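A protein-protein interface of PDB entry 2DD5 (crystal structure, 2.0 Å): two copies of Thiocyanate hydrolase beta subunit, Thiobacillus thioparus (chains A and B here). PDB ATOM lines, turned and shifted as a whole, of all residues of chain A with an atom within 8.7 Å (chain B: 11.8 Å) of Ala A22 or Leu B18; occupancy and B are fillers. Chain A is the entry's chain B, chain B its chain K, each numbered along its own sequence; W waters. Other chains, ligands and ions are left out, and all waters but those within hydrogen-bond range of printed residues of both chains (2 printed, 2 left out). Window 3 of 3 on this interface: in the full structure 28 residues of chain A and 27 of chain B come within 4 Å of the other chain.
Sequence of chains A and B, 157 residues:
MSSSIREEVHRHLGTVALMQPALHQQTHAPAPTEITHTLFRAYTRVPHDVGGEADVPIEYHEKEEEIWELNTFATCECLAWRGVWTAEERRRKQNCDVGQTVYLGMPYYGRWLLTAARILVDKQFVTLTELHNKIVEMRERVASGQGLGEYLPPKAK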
ATOM      1  N   ALA A  17      -2.072 -13.324 -19.413  1.00  0.00           N
ATOM      2  CA  ALA A  17      -3.477 -13.038 -19.695  1.00  0.00           C
ATOM      3  C   ALA A  17      -4.147 -12.441 -18.457  1.00  0.00           C
ATOM      4  O   ALA A  17      -5.081 -11.652 -18.564  1.00  0.00           O
ATOM      5  CB  ALA A  17      -4.200 -14.315 -20.118  1.00  0.00           C
ATOM      6  N   LEU A  18      -3.666 -12.832 -17.282  1.00  0.00           N
ATOM      7  CA  LEU A  18      -4.209 -12.337 -16.020  1.00  0.00           C
ATOM      8  C   LEU A  18      -3.936 -10.851 -15.853  1.00  0.00           C
ATOM      9  O   LEU A  18      -4.660 -10.155 -15.137  1.00  0.00           O
ATOM     10  CB  LEU A  18      -3.579 -13.082 -14.841  1.00  0.00           C
ATOM     11  CG  LEU A  18      -3.765 -14.596 -14.744  1.00  0.00           C
ATOM     12  CD1 LEU A  18      -2.899 -15.145 -13.612  1.00  0.00           C
ATOM     13  CD2 LEU A  18      -5.227 -14.915 -14.492  1.00  0.00           C
ATOM     14  N   MET A  19      -2.897 -10.365 -16.522  1.00  0.00           N
ATOM     15  CA  MET A  19      -2.504  -8.965 -16.412  1.00  0.00           C
ATOM     16  C   MET A  19      -3.002  -8.081 -17.550  1.00  0.00           C
ATOM     17  O   MET A  19      -2.622  -6.912 -17.651  1.00  0.00           O
ATOM     18  CB  MET A  19      -0.981  -8.883 -16.306  1.00  0.00           C
ATOM     19  CG  MET A  19      -0.408  -9.952 -15.387  1.00  0.00           C
ATOM     20  SD  MET A  19       1.384 -10.012 -15.338  1.00  0.00           S
ATOM     21  CE  MET A  19       1.647 -10.715 -13.702  1.00  0.00           C
ATOM     22  N   GLN A  20      -3.852  -8.642 -18.406  1.00  0.00           N
ATOM     23  CA  GLN A  20      -4.425  -7.897 -19.525  1.00  0.00           C
ATOM     24  C   GLN A  20      -5.121  -6.653 -18.976  1.00  0.00           C
ATOM     25  O   GLN A  20      -6.089  -6.762 -18.222  1.00  0.00           O
ATOM     26  CB  GLN A  20      -5.441  -8.778 -20.267  1.00  0.00           C
ATOM     27  CG  GLN A  20      -6.390  -8.024 -21.193  1.00  0.00           C
ATOM     28  CD  GLN A  20      -5.682  -7.364 -22.359  1.00  0.00           C
ATOM     29  OE1 GLN A  20      -5.023  -8.033 -23.158  1.00  0.00           O
ATOM     30  NE2 GLN A  20      -5.820  -6.043 -22.467  1.00  0.00           N
ATOM     31  N   PRO A  21      -4.635  -5.455 -19.343  1.00  0.00           N
ATOM     32  CA  PRO A  21      -5.234  -4.206 -18.866  1.00  0.00           C
ATOM     33  C   PRO A  21      -6.713  -4.106 -19.221  1.00  0.00           C
ATOM     34  O   PRO A  21      -7.163  -4.652 -20.234  1.00  0.00           O
ATOM     35  CB  PRO A  21      -4.403  -3.134 -19.561  1.00  0.00           C
ATOM     36  CG  PRO A  21      -3.076  -3.794 -19.730  1.00  0.00           C
ATOM     37  CD  PRO A  21      -3.452  -5.178 -20.176  1.00  0.00           C
ATOM     38  N   ALA A  22      -7.462  -3.401 -18.386  1.00  0.00           N
ATOM     39  CA  ALA A  22      -8.882  -3.240 -18.618  1.00  0.00           C
ATOM     40  C   ALA A  22      -9.422  -2.074 -17.821  1.00  0.00           C
ATOM     41  O   ALA A  22      -8.759  -1.557 -16.919  1.00  0.00           O
ATOM     42  CB  ALA A  22      -9.618  -4.513 -18.213  1.00  0.00           C
ATOM     43  N   LEU A  23     -10.622  -1.644 -18.193  1.00  0.00           N
ATOM     44  CA  LEU A  23     -11.317  -0.592 -17.477  1.00  0.00           C
ATOM     45  C   LEU A  23     -12.325  -1.444 -16.706  1.00  0.00           C
ATOM     46  O   LEU A  23     -13.303  -1.933 -17.270  1.00  0.00           O
ATOM     47  CB  LEU A  23     -12.004   0.364 -18.453  1.00  0.00           C
ATOM     48  CG  LEU A  23     -11.022   1.183 -19.301  1.00  0.00           C
ATOM     49  CD1 LEU A  23     -11.783   2.133 -20.202  1.00  0.00           C
ATOM     50  CD2 LEU A  23     -10.081   1.969 -18.388  1.00  0.00           C
ATOM     51  N   HIS A  24     -12.031  -1.655 -15.426  1.00  0.00           N
ATOM     52  CA  HIS A  24     -12.832  -2.496 -14.539  1.00  0.00           C
ATOM     53  C   HIS A  24     -13.756  -1.672 -13.648  1.00  0.00           C
ATOM     54  O   HIS A  24     -13.295  -0.990 -12.733  1.00  0.00           O
ATOM     55  CB  HIS A  24     -11.883  -3.320 -13.666  1.00  0.00           C
ATOM     56  CG  HIS A  24     -12.556  -4.391 -12.864  1.00  0.00           C
ATOM     57  ND1 HIS A  24     -12.916  -5.608 -13.400  1.00  0.00           N
ATOM     58  CD2 HIS A  24     -12.899  -4.440 -11.554  1.00  0.00           C
ATOM     59  CE1 HIS A  24     -13.448  -6.362 -12.455  1.00  0.00           C
ATOM     60  NE2 HIS A  24     -13.449  -5.677 -11.325  1.00  0.00           N
ATOM     61  N   GLN A  25     -15.056  -1.742 -13.912  1.00  0.00           N
ATOM     62  CA  GLN A  25     -16.023  -0.990 -13.118  1.00  0.00           C
ATOM     63  C   GLN A  25     -16.872  -1.918 -12.262  1.00  0.00           C
ATOM     64  O   GLN A  25     -17.743  -2.620 -12.775  1.00  0.00           O
ATOM     65  CB  GLN A  25     -16.945  -0.180 -14.026  1.00  0.00           C
ATOM     66  CG  GLN A  25     -17.889   0.735 -13.260  1.00  0.00           C
ATOM     67  CD  GLN A  25     -19.286   0.729 -13.832  1.00  0.00           C
ATOM     68  OE1 GLN A  25     -19.493   1.054 -15.002  1.00  0.00           O
ATOM     69  NE2 GLN A  25     -20.261   0.354 -13.006  1.00  0.00           N
ATOM     70  N   GLN A  26     -16.620  -1.931 -10.959  1.00  0.00           N
ATOM     71  CA  GLN A  26     -17.403  -2.780 -10.074  1.00  0.00           C
ATOM     72  C   GLN A  26     -18.822  -2.237 -10.040  1.00  0.00           C
ATOM     73  O   GLN A  26     -19.039  -1.025 -10.091  1.00  0.00           O
ATOM     74  CB  GLN A  26     -16.841  -2.778  -8.653  1.00  0.00           C
ATOM     75  CG  GLN A  26     -15.408  -3.239  -8.521  1.00  0.00           C
ATOM     76  CD  GLN A  26     -15.076  -3.648  -7.096  1.00  0.00           C
ATOM     77  OE1 GLN A  26     -15.502  -3.000  -6.137  1.00  0.00           O
ATOM     78  NE2 GLN A  26     -14.310  -4.725  -6.951  1.00  0.00           N
ATOM     79  N   HIS B  10     -11.612  15.384  -8.940  1.00  0.00           N
ATOM     80  CA  HIS B  10     -12.423  14.296  -8.421  1.00  0.00           C
ATOM     81  C   HIS B  10     -12.809  13.277  -9.491  1.00  0.00           C
ATOM     82  O   HIS B  10     -12.921  12.090  -9.195  1.00  0.00           O
ATOM     83  CB  HIS B  10     -13.647  14.861  -7.709  1.00  0.00           C
ATOM     84  CG  HIS B  10     -13.299  15.613  -6.464  1.00  0.00           C
ATOM     85  ND1 HIS B  10     -12.628  15.028  -5.410  1.00  0.00           N
ATOM     86  CD2 HIS B  10     -13.474  16.913  -6.124  1.00  0.00           C
ATOM     87  CE1 HIS B  10     -12.402  15.936  -4.477  1.00  0.00           C
ATOM     88  NE2 HIS B  10     -12.904  17.087  -4.885  1.00  0.00           N
ATOM     89  N   ARG B  11     -13.000  13.726 -10.730  1.00  0.00           N
ATOM     90  CA  ARG B  11     -13.325  12.792 -11.802  1.00  0.00           C
ATOM     91  C   ARG B  11     -12.104  11.906 -12.020  1.00  0.00           C
ATOM     92  O   ARG B  11     -12.222  10.705 -12.264  1.00  0.00           O
ATOM     93  CB  ARG B  11     -13.648  13.523 -13.107  1.00  0.00           C
ATOM     94  CG  ARG B  11     -15.121  13.838 -13.296  1.00  0.00           C
ATOM     95  CD  ARG B  11     -15.465  13.968 -14.777  1.00  0.00           C
ATOM     96  NE  ARG B  11     -14.721  15.042 -15.426  1.00  0.00           N
ATOM     97  CZ  ARG B  11     -14.851  16.332 -15.124  1.00  0.00           C
ATOM     98  NH1 ARG B  11     -15.700  16.714 -14.179  1.00  0.00           N
ATOM     99  NH2 ARG B  11     -14.128  17.241 -15.766  1.00  0.00           N
ATOM    100  N   HIS B  12     -10.927  12.517 -11.925  1.00  0.00           N
ATOM    101  CA  HIS B  12      -9.678  11.791 -12.101  1.00  0.00           C
ATOM    102  C   HIS B  12      -9.521  10.720 -11.027  1.00  0.00           C
ATOM    103  O   HIS B  12      -9.208   9.572 -11.334  1.00  0.00           O
ATOM    104  CB  HIS B  12      -8.496  12.760 -12.052  1.00  0.00           C
ATOM    105  CG  HIS B  12      -7.162  12.094 -12.193  1.00  0.00           C
ATOM    106  ND1 HIS B  12      -6.506  11.507 -11.132  1.00  0.00           N
ATOM    107  CD2 HIS B  12      -6.366  11.912 -13.274  1.00  0.00           C
ATOM    108  CE1 HIS B  12      -5.362  10.994 -11.552  1.00  0.00           C
ATOM    109  NE2 HIS B  12      -5.253  11.226 -12.848  1.00  0.00           N
ATOM    110  N   LEU B  13      -9.746  11.094  -9.771  1.00  0.00           N
ATOM    111  CA  LEU B  13      -9.619  10.148  -8.667  1.00  0.00           C
ATOM    112  C   LEU B  13     -10.549   8.952  -8.851  1.00  0.00           C
ATOM    113  O   LEU B  13     -10.245   7.840  -8.408  1.00  0.00           O
ATOM    114  CB  LEU B  13      -9.914  10.842  -7.330  1.00  0.00           C
ATOM    115  CG  LEU B  13      -8.879  11.875  -6.867  1.00  0.00           C
ATOM    116  CD1 LEU B  13      -9.334  12.541  -5.575  1.00  0.00           C
ATOM    117  CD2 LEU B  13      -7.536  11.187  -6.660  1.00  0.00           C
ATOM    118  N   GLY B  14     -11.678   9.182  -9.516  1.00  0.00           N
ATOM    119  CA  GLY B  14     -12.624   8.105  -9.745  1.00  0.00           C
ATOM    120  C   GLY B  14     -12.272   7.247 -10.945  1.00  0.00           C
ATOM    121  O   GLY B  14     -12.470   6.032 -10.930  1.00  0.00           O
ATOM    122  N   THR B  15     -11.738   7.875 -11.987  1.00  0.00           N
ATOM    123  CA  THR B  15     -11.368   7.163 -13.206  1.00  0.00           C
ATOM    124  C   THR B  15     -10.187   6.215 -13.004  1.00  0.00           C
ATOM    125  O   THR B  15     -10.188   5.100 -13.528  1.00  0.00           O
ATOM    126  CB  THR B  15     -11.018   8.155 -14.339  1.00  0.00           C
ATOM    127  OG1 THR B  15     -12.102   9.072 -14.518  1.00  0.00           O
ATOM    128  CG2 THR B  15     -10.772   7.413 -15.649  1.00  0.00           C
ATOM    129  N   VAL B  16      -9.185   6.656 -12.248  1.00  0.00           N
ATOM    130  CA  VAL B  16      -8.006   5.830 -12.001  1.00  0.00           C
ATOM    131  C   VAL B  16      -8.382   4.503 -11.355  1.00  0.00           C
ATOM    132  O   VAL B  16      -7.659   3.510 -11.481  1.00  0.00           O
ATOM    133  CB  VAL B  16      -6.976   6.561 -11.099  1.00  0.00           C
ATOM    134  CG1 VAL B  16      -6.447   7.797 -11.815  1.00  0.00           C
ATOM    135  CG2 VAL B  16      -7.611   6.948  -9.780  1.00  0.00           C
ATOM    136  N   ALA B  17      -9.517   4.490 -10.668  1.00  0.00           N
ATOM    137  CA  ALA B  17      -9.993   3.280 -10.014  1.00  0.00           C
ATOM    138  C   ALA B  17     -10.282   2.192 -11.047  1.00  0.00           C
ATOM    139  O   ALA B  17     -10.140   1.006 -10.760  1.00  0.00           O
ATOM    140  CB  ALA B  17     -11.248   3.581  -9.204  1.00  0.00           C
ATOM    141  N   LEU B  18     -10.692   2.602 -12.245  1.00  0.00           N
ATOM    142  CA  LEU B  18     -10.995   1.655 -13.316  1.00  0.00           C
ATOM    143  C   LEU B  18      -9.737   0.933 -13.777  1.00  0.00           C
ATOM    144  O   LEU B  18      -9.796  -0.206 -14.245  1.00  0.00           O
ATOM    145  CB  LEU B  18     -11.604   2.382 -14.520  1.00  0.00           C
ATOM    146  CG  LEU B  18     -12.926   3.131 -14.354  1.00  0.00           C
ATOM    147  CD1 LEU B  18     -13.258   3.865 -15.647  1.00  0.00           C
ATOM    148  CD2 LEU B  18     -14.030   2.149 -13.999  1.00  0.00           C
ATOM    149  N   MET B  19      -8.597   1.607 -13.637  1.00  0.00           N
ATOM    150  CA  MET B  19      -7.318   1.062 -14.069  1.00  0.00           C
ATOM    151  C   MET B  19      -6.538   0.356 -12.972  1.00  0.00           C
ATOM    152  O   MET B  19      -5.373  -0.003 -13.168  1.00  0.00           O
ATOM    153  CB  MET B  19      -6.464   2.180 -14.657  1.00  0.00           C
ATOM    154  CG  MET B  19      -7.227   3.078 -15.606  1.00  0.00           C
ATOM    155  SD  MET B  19      -6.234   4.467 -16.152  1.00  0.00           S
ATOM    156  CE  MET B  19      -7.127   4.966 -17.631  1.00  0.00           C
ATOM    157  N   GLN B  20      -7.162   0.165 -11.815  1.00  0.00           N
ATOM    158  CA  GLN B  20      -6.492  -0.525 -10.720  1.00  0.00           C
ATOM    159  C   GLN B  20      -6.033  -1.880 -11.250  1.00  0.00           C
ATOM    160  O   GLN B  20      -6.851  -2.673 -11.720  1.00  0.00           O
ATOM    161  CB  GLN B  20      -7.458  -0.732  -9.550  1.00  0.00           C
ATOM    162  CG  GLN B  20      -7.020  -1.796  -8.543  1.00  0.00           C
ATOM    163  CD  GLN B  20      -5.727  -1.445  -7.817  1.00  0.00           C
ATOM    164  OE1 GLN B  20      -5.600  -0.362  -7.236  1.00  0.00           O
ATOM    165  NE2 GLN B  20      -4.765  -2.365  -7.838  1.00  0.00           N
ATOM    166  N   PRO B  21      -4.717  -2.153 -11.196  1.00  0.00           N
ATOM    167  CA  PRO B  21      -4.167  -3.424 -11.674  1.00  0.00           C
ATOM    168  C   PRO B  21      -4.756  -4.610 -10.927  1.00  0.00           C
ATOM    169  O   PRO B  21      -5.130  -4.504  -9.758  1.00  0.00           O
ATOM    170  CB  PRO B  21      -2.669  -3.272 -11.413  1.00  0.00           C
ATOM    171  CG  PRO B  21      -2.455  -1.810 -11.577  1.00  0.00           C
ATOM    172  CD  PRO B  21      -3.634  -1.216 -10.850  1.00  0.00           C
ATOM    173  N   ALA B  22      -4.827  -5.747 -11.603  1.00  0.00           N
ATOM    174  CA  ALA B  22      -5.375  -6.940 -10.983  1.00  0.00           C
ATOM    175  C   ALA B  22      -4.961  -8.190 -11.729  1.00  0.00           C
ATOM    176  O   ALA B  22      -4.496  -8.127 -12.868  1.00  0.00           O
ATOM    177  CB  ALA B  22      -6.898  -6.846 -10.955  1.00  0.00           C
ATOM    178  N   LEU B  23      -5.103  -9.329 -11.061  1.00  0.00           N
ATOM    179  CA  LEU B  23      -4.830 -10.615 -11.679  1.00  0.00           C
ATOM    180  C   LEU B  23      -6.258 -11.049 -11.961  1.00  0.00           C
ATOM    181  O   LEU B  23      -6.987 -11.465 -11.057  1.00  0.00           O
ATOM    182  CB  LEU B  23      -4.136 -11.563 -10.699  1.00  0.00           C
ATOM    183  CG  LEU B  23      -2.710 -11.126 -10.335  1.00  0.00           C
ATOM    184  CD1 LEU B  23      -2.074 -12.151  -9.405  1.00  0.00           C
ATOM    185  CD2 LEU B  23      -1.881 -10.972 -11.604  1.00  0.00           C
ATOM    186  N   HIS B  24      -6.659 -10.905 -13.220  1.00  0.00           N
ATOM    187  CA  HIS B  24      -8.018 -11.207 -13.646  1.00  0.00           C
ATOM    188  C   HIS B  24      -8.136 -12.569 -14.317  1.00  0.00           C
ATOM    189  O   HIS B  24      -7.692 -12.763 -15.449  1.00  0.00           O
ATOM    190  CB  HIS B  24      -8.487 -10.090 -14.581  1.00  0.00           C
ATOM    191  CG  HIS B  24      -9.953 -10.111 -14.873  1.00  0.00           C
ATOM    192  ND1 HIS B  24     -10.478 -10.673 -16.017  1.00  0.00           N
ATOM    193  CD2 HIS B  24     -11.006  -9.620 -14.178  1.00  0.00           C
ATOM    194  CE1 HIS B  24     -11.791 -10.525 -16.015  1.00  0.00           C
ATOM    195  NE2 HIS B  24     -12.136  -9.888 -14.910  1.00  0.00           N
ATOM    196  N   GLN B  25      -8.745 -13.507 -13.603  1.00  0.00           N
ATOM    197  CA  GLN B  25      -8.917 -14.865 -14.094  1.00  0.00           C
ATOM    198  C   GLN B  25     -10.354 -15.152 -14.519  1.00  0.00           C
ATOM    199  O   GLN B  25     -11.228 -15.346 -13.676  1.00  0.00           O
ATOM    200  CB  GLN B  25      -8.505 -15.853 -13.003  1.00  0.00           C
ATOM    201  CG  GLN B  25      -8.498 -17.309 -13.433  1.00  0.00           C
ATOM    202  CD  GLN B  25      -8.515 -18.257 -12.248  1.00  0.00           C
ATOM    203  OE1 GLN B  25      -7.783 -18.065 -11.278  1.00  0.00           O
ATOM    204  NE2 GLN B  25      -9.348 -19.289 -12.324  1.00  0.00           N
ATOM    205  N   GLN B  26     -10.602 -15.172 -15.825  1.00  0.00           N
ATOM    206  CA  GLN B  26     -11.939 -15.470 -16.323  1.00  0.00           C
ATOM    207  C   GLN B  26     -12.244 -16.929 -16.022  1.00  0.00           C
ATOM    208  O   GLN B  26     -11.382 -17.791 -16.167  1.00  0.00           O
ATOM    209  CB  GLN B  26     -12.019 -15.241 -17.828  1.00  0.00           C
ATOM    210  CG  GLN B  26     -11.883 -13.799 -18.250  1.00  0.00           C
ATOM    211  CD  GLN B  26     -11.875 -13.655 -19.753  1.00  0.00           C
ATOM    212  OE1 GLN B  26     -12.767 -14.159 -20.439  1.00  0.00           O
ATOM    213  NE2 GLN B  26     -10.864 -12.969 -20.280  1.00  0.00           N
ATOM    214  N   VAL B  56     -15.303   0.575   0.410  1.00  0.00           N
ATOM    215  CA  VAL B  56     -14.736   1.912   0.544  1.00  0.00           C
ATOM    216  C   VAL B  56     -15.711   2.944   1.088  1.00  0.00           C
ATOM    217  O   VAL B  56     -16.910   2.692   1.201  1.00  0.00           O
ATOM    218  CB  VAL B  56     -14.222   2.430  -0.823  1.00  0.00           C
ATOM    219  CG1 VAL B  56     -13.256   1.421  -1.439  1.00  0.00           C
ATOM    220  CG2 VAL B  56     -15.397   2.687  -1.763  1.00  0.00           C
HETATM  221  O   HOH W   1     -10.887  -1.484 -11.034  1.00  0.00           O
HETATM  222  O   HOH W   2      -7.522 -10.883 -17.856  1.00  0.00           O
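The backbone carbonyl oxygen (O) of Leu A18 lies within hydrogen-bond range of the backbone NH (N) of His B24 (2.9 Å).
The backbone NH of His A24 sits at hydrogen-bond distance from the backbone carbonyl oxygen of Leu B18, 2.9 Å away.
The backbone carbonyl oxygen (O) of Leu A18 sits close to the backbone carbonyl oxygen (O) of Ala B22 (3.0 Å).
O of Ala A22 lies close to O of Leu B18 (3.2 Å).
CA of Leu B23 touches O of Leu A18, 3.5 Å away.
Leu A18 touches Gln B25.
Leu B18 touches Leu A23.
Gln A25 touches Leu B18 (CB to CD2, 3.7 Å).
Of the printed residues of chain B, Leu A18 touches Ala B22, Leu B23, His B24 and Gln B25.
No residue of chain B comes within 4 Å of Pro A21.
Ala A22 touches one residue of chain B.
Of chain B, only Leu B18 (3.6 Å) comes within 4 Å of Leu A23.
Printed residues of chain B within 4 Å of His A24: Leu B18.
Of chain B, only Leu B18 comes within 4 Å of Gln A25.
Val B16 touches none of the printed residues of chain A.
No residue of chain A comes within 4 Å of Ala B17.
Of chain A, only Ala A22, Leu A23, His A24 and Gln A25 come within 4 Å of Leu B18.
Printed residues of chain A within 4 Å of Ala B22: Leu A18.
Of the printed residues of chain A, Leu B23 touches Leu A18.
Of the printed residues of chain A, His B24 touches Leu A18.
Printed residues of chain A within 4 Å of Gln B25: Leu A18 (3.7 Å).
Gln B26 touches none of the printed residues of chain A.
The nearest residue of chain A that does not touch Leu B18 is Gln A26 (5.7 Å).
The nearest printed residue of chain A that does not touch Ala B22 is Met A19 (4.2 Å).
Of the 18 printed residues of chain B, 5 touch a printed residue of chain A.
Printed residues of chain B that touch a printed residue of chain A: Leu B18, Ala B22, Leu B23, His B24 and Gln B25.
Of the 10 printed residues of chain A, 5 touch a printed residue of chain B.
Hydrophobic or aromatic side chains of chain A within 4 Å of the printed part of chain B: Leu A18 and His A24.
Among the printed residues, no Asp or Glu carboxylate lies within 4 Å of a Lys or Arg side-chain nitrogen of the other chain.
Leu A18 touches Ala B22, and with the chains exchanged Ala A22 touches Leu B18.
Leu A18 touches Leu B23, and with the chains exchanged Leu A23 touches Leu B18.
Leu A18 touches His B24, and with the chains exchanged His A24 touches Leu B18.
Leu A18 touches Gln B25, and with the chains exchanged Gln A25 touches Leu B18.
Of the 8 pairs that touch across the chains among the printed residues, 8 have their exchanged pair printed and touching as well.
Water W1 bridges O of Ala B17 (2.6 Å) and O of His A24 (3.0 Å).
Water W2 lies within hydrogen-bond range of O of Ala A17 and O of His B24.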
